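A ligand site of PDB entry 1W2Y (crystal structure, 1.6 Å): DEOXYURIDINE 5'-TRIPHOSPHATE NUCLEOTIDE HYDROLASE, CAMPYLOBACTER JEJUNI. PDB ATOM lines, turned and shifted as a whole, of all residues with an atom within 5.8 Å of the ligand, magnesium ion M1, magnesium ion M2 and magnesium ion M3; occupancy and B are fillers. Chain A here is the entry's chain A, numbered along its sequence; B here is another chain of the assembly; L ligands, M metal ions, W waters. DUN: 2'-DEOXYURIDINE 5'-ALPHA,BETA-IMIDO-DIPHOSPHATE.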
ATOM      1  N   GLN A  14      20.779 -15.318  14.582  1.00  0.00           N
ATOM      2  CA  GLN A  14      22.032 -15.328  13.777  1.00  0.00           C
ATOM      3  C   GLN A  14      23.115 -16.104  14.524  1.00  0.00           C
ATOM      4  O   GLN A  14      23.854 -16.902  13.921  1.00  0.00           O
ATOM      5  CB  GLN A  14      22.515 -13.937  13.456  1.00  0.00           C
ATOM      6  CG  GLN A  14      23.636 -13.985  12.411  1.00  0.00           C
ATOM      7  CD  GLN A  14      23.159 -14.515  11.050  1.00  0.00           C
ATOM      8  OE1 GLN A  14      22.100 -14.058  10.546  1.00  0.00           O
ATOM      9  NE2 GLN A  14      23.949 -15.461  10.436  1.00  0.00           N
ATOM     10  N   LEU A  17      22.285 -19.837  14.315  1.00  0.00           N
ATOM     11  CA  LEU A  17      22.549 -20.348  12.971  1.00  0.00           C
ATOM     12  C   LEU A  17      24.066 -20.460  12.700  1.00  0.00           C
ATOM     13  O   LEU A  17      24.523 -21.448  12.148  1.00  0.00           O
ATOM     14  CB  LEU A  17      21.946 -19.394  11.940  1.00  0.00           C
ATOM     15  CG  LEU A  17      22.286 -19.684  10.489  1.00  0.00           C
ATOM     16  CD1 LEU A  17      21.829 -21.023   9.985  1.00  0.00           C
ATOM     17  CD2 LEU A  17      21.730 -18.560   9.654  1.00  0.00           C
ATOM     18  N   ASN A  18      24.839 -19.444  13.110  1.00  0.00           N
ATOM     19  CA  ASN A  18      26.288 -19.478  12.906  1.00  0.00           C
ATOM     20  C   ASN A  18      26.923 -20.599  13.743  1.00  0.00           C
ATOM     21  O   ASN A  18      27.858 -21.281  13.288  1.00  0.00           O
ATOM     22  CB  ASN A  18      26.946 -18.141  13.205  1.00  0.00           C
ATOM     23  CG  ASN A  18      26.661 -17.091  12.118  1.00  0.00           C
ATOM     24  OD1 ASN A  18      26.057 -17.409  11.102  1.00  0.00           O
ATOM     25  ND2 ASN A  18      27.155 -15.857  12.316  1.00  0.00           N
ATOM     26  N   THR A  21      26.024 -23.846  11.942  1.00  0.00           N
ATOM     27  CA  THR A  21      26.693 -23.930  10.621  1.00  0.00           C
ATOM     28  C   THR A  21      28.200 -24.119  10.764  1.00  0.00           C
ATOM     29  O   THR A  21      28.825 -24.935  10.060  1.00  0.00           O
ATOM     30  CB  THR A  21      26.408 -22.638   9.806  1.00  0.00           C
ATOM     31  OG1 THR A  21      24.978 -22.471   9.559  1.00  0.00           O
ATOM     32  CG2 THR A  21      27.098 -22.654   8.400  1.00  0.00           C
ATOM     33  N   ASN A  22      28.812 -23.321  11.632  1.00  0.00           N
ATOM     34  CA  ASN A  22      30.270 -23.175  11.697  1.00  0.00           C
ATOM     35  C   ASN A  22      30.981 -23.786  12.896  1.00  0.00           C
ATOM     36  O   ASN A  22      32.224 -23.837  12.955  1.00  0.00           O
ATOM     37  CB  ASN A  22      30.560 -21.701  11.722  1.00  0.00           C
ATOM     38  CG  ASN A  22      29.998 -20.998  10.514  1.00  0.00           C
ATOM     39  OD1 ASN A  22      30.203 -21.432   9.381  1.00  0.00           O
ATOM     40  ND2 ASN A  22      29.248 -19.908  10.765  1.00  0.00           N
ATOM     41  N   TRP A  39      33.336 -12.167   6.781  1.00  0.00           N
ATOM     42  CA  TRP A  39      31.979 -11.640   6.680  1.00  0.00           C
ATOM     43  C   TRP A  39      31.899 -10.482   5.668  1.00  0.00           C
ATOM     44  O   TRP A  39      30.877 -10.319   4.990  1.00  0.00           O
ATOM     45  CB  TRP A  39      31.492 -11.156   8.009  1.00  0.00           C
ATOM     46  CG  TRP A  39      31.428 -12.252   9.024  1.00  0.00           C
ATOM     47  CD1 TRP A  39      32.091 -12.286  10.186  1.00  0.00           C
ATOM     48  CD2 TRP A  39      30.686 -13.477   8.949  1.00  0.00           C
ATOM     49  NE1 TRP A  39      31.819 -13.437  10.889  1.00  0.00           N
ATOM     50  CE2 TRP A  39      30.954 -14.202  10.147  1.00  0.00           C
ATOM     51  CE3 TRP A  39      29.812 -14.034   8.017  1.00  0.00           C
ATOM     52  CZ2 TRP A  39      30.348 -15.425  10.437  1.00  0.00           C
ATOM     53  CZ3 TRP A  39      29.241 -15.318   8.261  1.00  0.00           C
ATOM     54  CH2 TRP A  39      29.509 -15.980   9.492  1.00  0.00           C
ATOM     55  N   CYS A  42      31.556 -11.986   2.360  1.00  0.00           N
ATOM     56  CA  CYS A  42      30.167 -12.477   2.250  1.00  0.00           C
ATOM     57  C   CYS A  42      29.224 -11.336   1.819  1.00  0.00           C
ATOM     58  O   CYS A  42      28.336 -11.514   0.982  1.00  0.00           O
ATOM     59  CB  CYS A  42      29.743 -13.084   3.595  1.00  0.00           C
ATOM     60  SG  CYS A  42      30.564 -14.637   3.963  1.00  0.00           S
ATOM     61  N   MET A  45      29.742 -10.022  -1.798  1.00  0.00           N
ATOM     62  CA  MET A  45      29.262 -11.041  -2.778  1.00  0.00           C
ATOM     63  C   MET A  45      27.734 -10.990  -2.845  1.00  0.00           C
ATOM     64  O   MET A  45      27.134 -11.129  -3.927  1.00  0.00           O
ATOM     65  CB  MET A  45      29.820 -12.401  -2.437  1.00  0.00           C
ATOM     66  CG  MET A  45      31.319 -12.503  -2.656  1.00  0.00           C
ATOM     67  SD  MET A  45      31.821 -12.254  -4.370  1.00  0.00           S
ATOM     68  CE  MET A  45      31.301 -13.848  -5.012  1.00  0.00           C
ATOM     69  N   GLU A  46      27.043 -10.791  -1.704  1.00  0.00           N
ATOM     70  CA  GLU A  46      25.567 -10.623  -1.769  1.00  0.00           C
ATOM     71  C   GLU A  46      25.229  -9.303  -2.431  1.00  0.00           C
ATOM     72  O   GLU A  46      24.192  -9.188  -3.073  1.00  0.00           O
ATOM     73  CB  GLU A  46      24.938 -10.709  -0.389  1.00  0.00           C
ATOM     74  CG  GLU A  46      25.111 -12.077   0.302  1.00  0.00           C
ATOM     75  CD  GLU A  46      24.478 -13.212  -0.461  1.00  0.00           C
ATOM     76  OE1 GLU A  46      23.353 -12.985  -1.046  1.00  0.00           O
ATOM     77  OE2 GLU A  46      25.044 -14.324  -0.439  1.00  0.00           O
ATOM     78  N   GLU A  49      24.957 -10.018  -5.977  1.00  0.00           N
ATOM     79  CA  GLU A  49      23.656 -10.628  -6.237  1.00  0.00           C
ATOM     80  C   GLU A  49      22.550  -9.609  -6.259  1.00  0.00           C
ATOM     81  O   GLU A  49      21.655  -9.696  -7.092  1.00  0.00           O
ATOM     82  CB  GLU A  49      23.310 -11.652  -5.169  1.00  0.00           C
ATOM     83  CG  GLU A  49      24.202 -12.898  -5.227  1.00  0.00           C
ATOM     84  CD  GLU A  49      23.845 -13.834  -4.090  1.00  0.00           C
ATOM     85  OE1 GLU A  49      24.786 -14.291  -3.419  1.00  0.00           O
ATOM     86  OE2 GLU A  49      22.629 -14.042  -3.830  1.00  0.00           O
ATOM     87  N   ASN A  70      13.588 -10.546  -5.612  1.00  0.00           N
ATOM     88  CA  ASN A  70      14.959 -10.944  -5.310  1.00  0.00           C
ATOM     89  C   ASN A  70      15.687  -9.832  -4.601  1.00  0.00           C
ATOM     90  O   ASN A  70      16.519 -10.085  -3.752  1.00  0.00           O
ATOM     91  CB  ASN A  70      15.747 -11.379  -6.543  1.00  0.00           C
ATOM     92  CG  ASN A  70      16.923 -12.260  -6.139  1.00  0.00           C
ATOM     93  OD1 ASN A  70      16.690 -13.356  -5.583  1.00  0.00           O
ATOM     94  ND2 ASN A  70      18.153 -11.773  -6.308  1.00  0.00           N
ATOM     95  N   ILE A  73      15.180 -10.499  -0.952  1.00  0.00           N
ATOM     96  CA  ILE A  73      16.015 -11.644  -0.533  1.00  0.00           C
ATOM     97  C   ILE A  73      17.495 -11.241  -0.329  1.00  0.00           C
ATOM     98  O   ILE A  73      18.114 -11.599   0.664  1.00  0.00           O
ATOM     99  CB  ILE A  73      15.936 -12.722  -1.622  1.00  0.00           C
ATOM    100  CG1 ILE A  73      14.539 -13.390  -1.635  1.00  0.00           C
ATOM    101  CG2 ILE A  73      17.043 -13.665  -1.570  1.00  0.00           C
ATOM    102  CD1 ILE A  73      14.031 -13.987  -0.276  1.00  0.00           C
ATOM    103  N   GLU A  74      18.049 -10.462  -1.266  1.00  0.00           N
ATOM    104  CA  GLU A  74      19.466 -10.141  -1.168  1.00  0.00           C
ATOM    105  C   GLU A  74      19.712  -9.145  -0.025  1.00  0.00           C
ATOM    106  O   GLU A  74      20.750  -9.209   0.663  1.00  0.00           O
ATOM    107  CB  GLU A  74      20.045  -9.675  -2.483  1.00  0.00           C
ATOM    108  CG  GLU A  74      19.776 -10.585  -3.639  1.00  0.00           C
ATOM    109  CD  GLU A  74      20.260 -12.026  -3.477  1.00  0.00           C
ATOM    110  OE1 GLU A  74      20.911 -12.364  -2.461  1.00  0.00           O
ATOM    111  OE2 GLU A  74      20.006 -12.817  -4.419  1.00  0.00           O
ATOM    112  N   VAL A  76      18.094  -9.161   2.686  1.00  0.00           N
ATOM    113  CA  VAL A  76      18.064 -10.038   3.861  1.00  0.00           C
ATOM    114  C   VAL A  76      19.334 -10.881   4.005  1.00  0.00           C
ATOM    115  O   VAL A  76      19.834 -11.067   5.143  1.00  0.00           O
ATOM    116  CB  VAL A  76      16.797 -10.902   3.792  1.00  0.00           C
ATOM    117  CG1 VAL A  76      16.864 -12.014   4.759  1.00  0.00           C
ATOM    118  CG2 VAL A  76      15.558  -9.966   4.048  1.00  0.00           C
ATOM    119  N   ASP A  77      19.892 -11.348   2.884  1.00  0.00           N
ATOM    120  CA  ASP A  77      21.166 -12.070   2.937  1.00  0.00           C
ATOM    121  C   ASP A  77      22.300 -11.162   3.477  1.00  0.00           C
ATOM    122  O   ASP A  77      23.095 -11.543   4.336  1.00  0.00           O
ATOM    123  CB  ASP A  77      21.553 -12.614   1.561  1.00  0.00           C
ATOM    124  CG  ASP A  77      20.723 -13.785   1.120  1.00  0.00           C
ATOM    125  OD1 ASP A  77      20.016 -14.364   1.976  1.00  0.00           O
ATOM    126  OD2 ASP A  77      20.720 -14.186  -0.069  1.00  0.00           O
ATOM    127  N   HIS A  80      22.001 -10.935   7.273  1.00  0.00           N
ATOM    128  CA  HIS A  80      22.547 -12.097   7.984  1.00  0.00           C
ATOM    129  C   HIS A  80      24.051 -11.868   8.229  1.00  0.00           C
ATOM    130  O   HIS A  80      24.592 -12.134   9.337  1.00  0.00           O
ATOM    131  CB  HIS A  80      22.403 -13.409   7.204  1.00  0.00           C
ATOM    132  CG  HIS A  80      21.061 -14.085   7.293  1.00  0.00           C
ATOM    133  ND1 HIS A  80      19.934 -13.594   6.669  1.00  0.00           N
ATOM    134  CD2 HIS A  80      20.696 -15.264   7.886  1.00  0.00           C
ATOM    135  CE1 HIS A  80      18.937 -14.459   6.840  1.00  0.00           C
ATOM    136  NE2 HIS A  80      19.356 -15.462   7.607  1.00  0.00           N
ATOM    137  N   PHE A  81      24.735 -11.351   7.194  1.00  0.00           N
ATOM    138  CA  PHE A  81      26.164 -11.165   7.312  1.00  0.00           C
ATOM    139  C   PHE A  81      26.557  -9.948   8.122  1.00  0.00           C
ATOM    140  O   PHE A  81      27.580  -9.948   8.845  1.00  0.00           O
ATOM    141  CB  PHE A  81      26.784 -11.185   5.923  1.00  0.00           C
ATOM    142  CG  PHE A  81      26.650 -12.513   5.210  1.00  0.00           C
ATOM    143  CD1 PHE A  81      27.090 -13.683   5.827  1.00  0.00           C
ATOM    144  CD2 PHE A  81      26.090 -12.621   3.925  1.00  0.00           C
ATOM    145  CE1 PHE A  81      27.076 -14.897   5.194  1.00  0.00           C
ATOM    146  CE2 PHE A  81      26.055 -13.840   3.296  1.00  0.00           C
ATOM    147  CZ  PHE A  81      26.528 -14.974   3.941  1.00  0.00           C
ATOM    148  N   SER A  84      26.206 -11.055  11.631  1.00  0.00           N
ATOM    149  CA  SER A  84      27.400 -11.866  11.907  1.00  0.00           C
ATOM    150  C   SER A  84      28.593 -10.989  12.262  1.00  0.00           C
ATOM    151  O   SER A  84      29.279 -11.230  13.265  1.00  0.00           O
ATOM    152  CB  SER A  84      27.671 -12.793  10.753  1.00  0.00           C
ATOM    153  OG  SER A  84      26.602 -13.721  10.519  1.00  0.00           O
ATOM    154  N   LYS A 175      14.289 -16.695   5.754  1.00  0.00           N
ATOM    155  CA  LYS A 175      15.583 -17.051   5.178  1.00  0.00           C
ATOM    156  C   LYS A 175      16.490 -17.766   6.225  1.00  0.00           C
ATOM    157  O   LYS A 175      17.205 -18.682   5.860  1.00  0.00           O
ATOM    158  CB  LYS A 175      16.271 -15.830   4.566  1.00  0.00           C
ATOM    159  CG  LYS A 175      17.607 -16.153   3.799  1.00  0.00           C
ATOM    160  CD  LYS A 175      17.525 -17.353   2.842  1.00  0.00           C
ATOM    161  CE  LYS A 175      18.770 -17.602   1.985  1.00  0.00           C
ATOM    162  NZ  LYS A 175      18.928 -16.612   0.912  1.00  0.00           N
ATOM    163  N   ASN A 179      18.218 -21.268   5.575  1.00  0.00           N
ATOM    164  CA  ASN A 179      19.640 -21.441   5.824  1.00  0.00           C
ATOM    165  C   ASN A 179      19.958 -22.699   6.658  1.00  0.00           C
ATOM    166  O   ASN A 179      20.912 -23.436   6.364  1.00  0.00           O
ATOM    167  CB  ASN A 179      20.239 -20.188   6.459  1.00  0.00           C
ATOM    168  CG  ASN A 179      20.447 -19.081   5.461  1.00  0.00           C
ATOM    169  OD1 ASN A 179      20.754 -19.362   4.293  1.00  0.00           O
ATOM    170  ND2 ASN A 179      20.291 -17.806   5.900  1.00  0.00           N
ATOM    171  N   ARG A 182      19.086 -25.798   4.389  1.00  0.00           N
ATOM    172  CA  ARG A 182      20.204 -26.077   3.479  1.00  0.00           C
ATOM    173  C   ARG A 182      21.297 -26.882   4.181  1.00  0.00           C
ATOM    174  O   ARG A 182      21.799 -27.851   3.651  1.00  0.00           O
ATOM    175  CB  ARG A 182      20.810 -24.745   3.018  1.00  0.00           C
ATOM    176  CG  ARG A 182      20.014 -24.045   1.945  1.00  0.00           C
ATOM    177  CD  ARG A 182      20.570 -22.661   1.661  1.00  0.00           C
ATOM    178  NE  ARG A 182      19.957 -21.954   0.550  1.00  0.00           N
ATOM    179  CZ  ARG A 182      20.231 -20.707   0.248  1.00  0.00           C
ATOM    180  NH1 ARG A 182      21.172 -20.023   0.935  1.00  0.00           N
ATOM    181  NH2 ARG A 182      19.616 -20.115  -0.754  1.00  0.00           N
ATOM    182  N   TYR A 187      24.199 -28.913   2.035  1.00  0.00           N
ATOM    183  CA  TYR A 187      24.789 -27.700   1.476  1.00  0.00           C
ATOM    184  C   TYR A 187      26.341 -27.744   1.475  1.00  0.00           C
ATOM    185  O   TYR A 187      26.981 -27.295   0.497  1.00  0.00           O
ATOM    186  CB  TYR A 187      24.301 -26.425   2.205  1.00  0.00           C
ATOM    187  CG  TYR A 187      24.154 -25.205   1.306  1.00  0.00           C
ATOM    188  CD1 TYR A 187      23.280 -25.221   0.230  1.00  0.00           C
ATOM    189  CD2 TYR A 187      24.852 -24.057   1.577  1.00  0.00           C
ATOM    190  CE1 TYR A 187      23.103 -24.107  -0.540  1.00  0.00           C
ATOM    191  CE2 TYR A 187      24.690 -22.934   0.793  1.00  0.00           C
ATOM    192  CZ  TYR A 187      23.822 -22.958  -0.282  1.00  0.00           C
ATOM    193  OH  TYR A 187      23.678 -21.841  -1.107  1.00  0.00           O
ATOM    194  N   LYS A 194      19.694 -26.835  -5.157  1.00  0.00           N
ATOM    195  CA  LYS A 194      19.270 -25.453  -4.928  1.00  0.00           C
ATOM    196  C   LYS A 194      18.072 -25.044  -5.804  1.00  0.00           C
ATOM    197  O   LYS A 194      17.358 -24.084  -5.484  1.00  0.00           O
ATOM    198  CB  LYS A 194      20.426 -24.471  -5.096  1.00  0.00           C
ATOM    199  CG  LYS A 194      20.199 -23.161  -4.347  1.00  0.00           C
ATOM    200  CD  LYS A 194      21.368 -22.275  -4.392  1.00  0.00           C
ATOM    201  CE  LYS A 194      21.134 -20.957  -3.644  1.00  0.00           C
ATOM    202  NZ  LYS A 194      21.606 -19.820  -4.422  1.00  0.00           N
ATOM    203  N   ASP A 201      15.456 -22.217  -4.473  1.00  0.00           N
ATOM    204  CA  ASP A 201      14.931 -22.311  -3.120  1.00  0.00           C
ATOM    205  C   ASP A 201      14.426 -20.965  -2.547  1.00  0.00           C
ATOM    206  O   ASP A 201      13.366 -20.914  -1.908  1.00  0.00           O
ATOM    207  CB  ASP A 201      15.876 -23.075  -2.197  1.00  0.00           C
ATOM    208  CG  ASP A 201      17.267 -22.432  -2.028  1.00  0.00           C
ATOM    209  OD1 ASP A 201      17.574 -21.303  -2.559  1.00  0.00           O
ATOM    210  OD2 ASP A 201      18.095 -23.002  -1.292  1.00  0.00           O
ATOM    211  N   ASN A 202      15.142 -19.878  -2.847  1.00  0.00           N
ATOM    212  CA  ASN A 202      14.712 -18.563  -2.408  1.00  0.00           C
ATOM    213  C   ASN A 202      13.332 -18.197  -2.931  1.00  0.00           C
ATOM    214  O   ASN A 202      12.575 -17.514  -2.228  1.00  0.00           O
ATOM    215  CB  ASN A 202      15.702 -17.494  -2.851  1.00  0.00           C
ATOM    216  CG  ASN A 202      17.001 -17.556  -2.059  1.00  0.00           C
ATOM    217  OD1 ASN A 202      16.945 -17.567  -0.823  1.00  0.00           O
ATOM    218  ND2 ASN A 202      18.170 -17.641  -2.739  1.00  0.00           N
ATOM    219  N   LYS B  57      33.501 -19.950  -0.125  1.00  0.00           N
ATOM    220  CA  LYS B  57      32.439 -20.002   0.851  1.00  0.00           C
ATOM    221  C   LYS B  57      32.792 -20.991   1.934  1.00  0.00           C
ATOM    222  O   LYS B  57      33.218 -22.124   1.649  1.00  0.00           O
ATOM    223  CB  LYS B  57      31.109 -20.404   0.182  1.00  0.00           C
ATOM    224  CG  LYS B  57      30.477 -19.316  -0.688  1.00  0.00           C
ATOM    225  CD  LYS B  57      29.087 -19.668  -1.135  1.00  0.00           C
ATOM    226  CE  LYS B  57      28.426 -18.581  -1.898  1.00  0.00           C
ATOM    227  NZ  LYS B  57      27.064 -18.882  -2.416  1.00  0.00           N
ATOM    228  N   HIS B  58      32.636 -20.593   3.199  1.00  0.00           N
ATOM    229  CA  HIS B  58      32.987 -21.455   4.307  1.00  0.00           C
ATOM    230  C   HIS B  58      31.866 -22.435   4.702  1.00  0.00           C
ATOM    231  O   HIS B  58      32.007 -23.227   5.638  1.00  0.00           O
ATOM    232  CB  HIS B  58      33.402 -20.641   5.544  1.00  0.00           C
ATOM    233  CG  HIS B  58      32.347 -19.705   6.026  1.00  0.00           C
ATOM    234  ND1 HIS B  58      32.273 -18.372   5.621  1.00  0.00           N
ATOM    235  CD2 HIS B  58      31.301 -19.908   6.878  1.00  0.00           C
ATOM    236  CE1 HIS B  58      31.223 -17.816   6.220  1.00  0.00           C
ATOM    237  NE2 HIS B  58      30.627 -18.725   6.990  1.00  0.00           N
ATOM    238  N   TRP B  59      30.704 -22.259   4.041  1.00  0.00           N
ATOM    239  CA  TRP B  59      29.501 -22.982   4.385  1.00  0.00           C
ATOM    240  C   TRP B  59      28.879 -23.818   3.277  1.00  0.00           C
ATOM    241  O   TRP B  59      27.788 -24.375   3.488  1.00  0.00           O
ATOM    242  CB  TRP B  59      28.415 -22.001   4.887  1.00  0.00           C
ATOM    243  CG  TRP B  59      27.850 -21.100   3.838  1.00  0.00           C
ATOM    244  CD1 TRP B  59      26.654 -21.261   3.158  1.00  0.00           C
ATOM    245  CD2 TRP B  59      28.405 -19.867   3.381  1.00  0.00           C
ATOM    246  NE1 TRP B  59      26.466 -20.210   2.284  1.00  0.00           N
ATOM    247  CE2 TRP B  59      27.537 -19.348   2.401  1.00  0.00           C
ATOM    248  CE3 TRP B  59      29.595 -19.159   3.672  1.00  0.00           C
ATOM    249  CZ2 TRP B  59      27.763 -18.109   1.781  1.00  0.00           C
ATOM    250  CZ3 TRP B  59      29.824 -17.963   3.033  1.00  0.00           C
ATOM    251  CH2 TRP B  59      28.927 -17.452   2.069  1.00  0.00           C
ATOM    252  N   LYS B  60      29.531 -23.879   2.119  1.00  0.00           N
ATOM    253  CA  LYS B  60      28.902 -24.477   0.938  1.00  0.00           C
ATOM    254  C   LYS B  60      29.950 -25.180   0.133  1.00  0.00           C
ATOM    255  O   LYS B  60      30.986 -24.593  -0.207  1.00  0.00           O
ATOM    256  CB  LYS B  60      28.259 -23.407   0.033  1.00  0.00           C
ATOM    257  CG  LYS B  60      27.408 -23.979  -1.106  1.00  0.00           C
ATOM    258  CD  LYS B  60      26.887 -22.874  -2.043  1.00  0.00           C
ATOM    259  CE  LYS B  60      25.947 -23.462  -3.085  1.00  0.00           C
ATOM    260  NZ  LYS B  60      25.435 -22.462  -4.095  1.00  0.00           N
HETATM  261  N1  DUN L   1      24.948 -17.751   6.114  1.00  0.00           N
HETATM  262  C2  DUN L   1      24.943 -17.469   7.466  1.00  0.00           C
HETATM  263  N3  DUN L   1      26.019 -17.788   8.199  1.00  0.00           N
HETATM  264  C4  DUN L   1      27.136 -18.374   7.687  1.00  0.00           C
HETATM  265  C5  DUN L   1      27.154 -18.649   6.312  1.00  0.00           C
HETATM  266  C6  DUN L   1      26.042 -18.348   5.587  1.00  0.00           C
HETATM  267  O2  DUN L   1      23.915 -16.907   7.945  1.00  0.00           O
HETATM  268  O4  DUN L   1      28.108 -18.654   8.406  1.00  0.00           O
HETATM  269  C1' DUN L   1      23.767 -17.448   5.311  1.00  0.00           C
HETATM  270  C2' DUN L   1      23.376 -15.981   5.249  1.00  0.00           C
HETATM  271  C3' DUN L   1      22.704 -15.847   3.909  1.00  0.00           C
HETATM  272  C4' DUN L   1      23.038 -17.148   3.138  1.00  0.00           C
HETATM  273  O4' DUN L   1      23.936 -17.894   3.965  1.00  0.00           O
HETATM  274  O3' DUN L   1      21.274 -15.753   4.115  1.00  0.00           O
HETATM  275  C5' DUN L   1      23.647 -16.967   1.772  1.00  0.00           C
HETATM  276  O5' DUN L   1      23.928 -18.292   1.222  1.00  0.00           O
HETATM  277  PA  DUN L   1      24.448 -18.417  -0.283  1.00  0.00           P
HETATM  278  O1A DUN L   1      25.285 -17.205  -0.632  1.00  0.00           O
HETATM  279  O2A DUN L   1      25.099 -19.772  -0.288  1.00  0.00           O
HETATM  280  PB  DUN L   1      22.018 -17.311  -1.545  1.00  0.00           P
HETATM  281  O1B DUN L   1      21.126 -17.401  -0.277  1.00  0.00           O
HETATM  282  O2B DUN L   1      21.265 -17.650  -2.774  1.00  0.00           O
HETATM  283  O3B DUN L   1      22.760 -15.971  -1.620  1.00  0.00           O
HETATM  284  N3A DUN L   1      23.093 -18.537  -1.288  1.00  0.00           N
HETATM  285 MG    MG M   1      24.853 -15.724  -1.892  1.00  0.00          MG
HETATM  286 MG    MG M   2      21.866 -14.098  -1.860  1.00  0.00          MG
HETATM  287 MG    MG M   3      20.887 -14.669  -4.920  1.00  0.00          MG
HETATM  288  O   HOH W   1      21.472 -16.606  -5.159  1.00  0.00           O
HETATM  289  O   HOH W   2      18.785 -15.173  -5.545  1.00  0.00           O
HETATM  290  O   HOH W   3      20.206 -15.110  -2.859  1.00  0.00           O
HETATM  291  O   HOH W   4      27.070 -15.615  -2.173  1.00  0.00           O
HETATM  292  O   HOH W   5      24.148 -20.687   7.274  1.00  0.00           O
HETATM  293  O   HOH W   6      21.339 -14.300  -6.687  1.00  0.00           O
HETATM  294  O   HOH W   7      24.418 -19.978  -4.114  1.00  0.00           O
HETATM  295  O   HOH W   8      24.975 -17.153  -3.561  1.00  0.00           O
HETATM  296  O   HOH W   9      23.011 -20.510   3.157  1.00  0.00           O
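Water W8 bridges NZ of Lys 57 of chain B (2.9 Å) and N3A of the ligand (3.3 Å).
Water W3 lies within hydrogen-bond range of O2B of the ligand (2.8 Å) and ND2 of Asn 202 (3.3 Å).
Water W1 bridges an oxygen (O2B) of the ligand and the side-chain amino group (NZ) of Lys 194.
Water W9 lies within hydrogen-bond range of the side-chain amide oxygen (OD1) of Asn 179 (2.8 Å), an oxygen (O4') of the ligand (2.9 Å) and the guanidinium group (NH1) of Arg 182 (2.9 Å).
Magnesium ion M2 is bound by the side-chain carboxylate (OE1) of Glu 46 (2.0 Å).
Magnesium ion M2 is bound by OE1 of Glu 74, 2.1 Å away.
Magnesium ion M2 is bound by an oxygen (O3B) of the ligand, 2.1 Å away.
OE2 of Glu 49 binds magnesium ion M2 (2.1 Å).
OD2 of Asp 77 binds magnesium ion M2 (2.1 Å).
Magnesium ion M2 is bound by water W3, 2.2 Å away.
Magnesium ion M2 has six donor atoms within binding distance.
Magnesium ion M3 is bound by water W6 (1.9 Å), water W1 (2.0 Å), the side-chain carboxylate of Glu 74 (2.1 Å), the side-chain carboxylate of Glu 49 (2.1 Å), water W3 (2.2 Å) and water W2 (2.3 Å).
Magnesium ion M3 has six donor atoms within binding distance.
Within 4 Å of magnesium ion M3: Glu 49 and Glu 74.
Magnesium ion M1 is bound by an oxygen (O1A) of the ligand, at 2.0 Å.
OE2 of Glu 46 binds magnesium ion M1, at 2.0 Å.
OE1 of Glu 49 binds magnesium ion M1, at 2.1 Å.
O3B of the ligand is bound to magnesium ion M1 (2.1 Å).
Magnesium ion M1 is bound by water W8 (2.2 Å).
Magnesium ion M1 is bound by water W4 (2.2 Å).
Magnesium ion M1 has six donor atoms within binding distance.
Merely in contact with magnesium ion M1: Lys 57 of chain B.
The nearest printed residue that does not touch magnesium ion M1 is Asp 77 (4.8 Å).
ND2 of Asn 179 is in hydrogen-bond range of O3' of the ligand, at 2.9 Å.
ND2 of Asn 22 lies within hydrogen-bond range of O4 of the ligand, at 2.9 Å.
ND2 of Asn 202 lies within hydrogen-bond range of O2B of the ligand (3.1 Å).
An oxygen (O2B) of the ligand lies within salt-bridge range of the side-chain amino group (NZ) of Lys 194, 2.7 Å away.
The indole nitrogen (NE1) of Trp 59 of chain B lies within hydrogen-bond range of an oxygen (O2A) of the ligand (2.9 Å).
The guanidinium group of Arg 182 lies within salt-bridge range of an oxygen (O1B) of the ligand, at 2.9 Å.
The side-chain amino group (NZ) of Lys 175 lies within salt-bridge range of an oxygen (O1B) of the ligand, at 2.6 Å.
NE2 of Gln 14 is in hydrogen-bond range of O2 of the ligand, at 2.9 Å.
O4 of the ligand lies within hydrogen-bond range of NE2 of His 58 of chain B, at 2.9 Å.
The side-chain amide oxygen (OD1) of Asn 18 is in hydrogen-bond range of a nitrogen (N3) of the ligand.
O2A of the ligand is in hydrogen-bond range of OH of Tyr 187.
The side-chain amino group (NZ) of Lys 57 of chain B lies within salt-bridge range of an oxygen (O2A) of the ligand, at 3.0 Å.
Residues that only touch the ligand: Leu 17 (3.2 Å), Trp 39 (3.2 Å), His 80 (3.4 Å), Phe 81 (3.6 Å) and Lys 60 of chain B (3.99 Å).
Hydrophobic or aromatic side chains that line the ligand: Leu 17, Trp 39, His 80, Phe 81, Tyr 187, His 58 of chain B and Trp 59 of chain B.
20 residues have an atom within 4 Å of the ligand: Gln 14, Leu 17, Asn 18, Asn 22, Trp 39, Glu 46, Glu 49, Asp 77, His 80, Phe 81, Lys 175, Asn 179, Arg 182, Tyr 187, Lys 194, Asn 202, Lys 57 of chain B, His 58 of chain B, Trp 59 of chain B and Lys 60 of chain B.
The nearest printed residue that does not touch the ligand is Thr 21 (4.1 Å).
The guanidinium group of Arg 182 lies close to the side-chain amide nitrogen of Asn 202 (3.5 Å).
NE2 of Gln 14 lies within hydrogen-bond range of OD1 of Asn 18, 2.9 Å away.
NZ of Lys 175 sits at hydrogen-bond distance from OD1 of Asn 202, at 2.8 Å.
O of Arg 182 is in hydrogen-bond range of N of Tyr 187 (3.1 Å).
ND2 of Asn 22 lies close to O of Asn 18 (3.2 Å).
NE2 of Gln 14 lies within hydrogen-bond range of OG of Ser 84 (3.2 Å).
NE of Arg 182 lies within salt-bridge range of OD2 of Asp 201 (2.8 Å).
The side-chain hydroxyl of Ser 84 sits at hydrogen-bond distance from the backbone carbonyl oxygen of His 80 (2.8 Å).
Within 4 Å of magnesium ion M2: Glu 46, Glu 49, Glu 74 and Asp 77.
The nearest printed residue that does not touch magnesium ion M2 is Lys 175 (4.8 Å).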
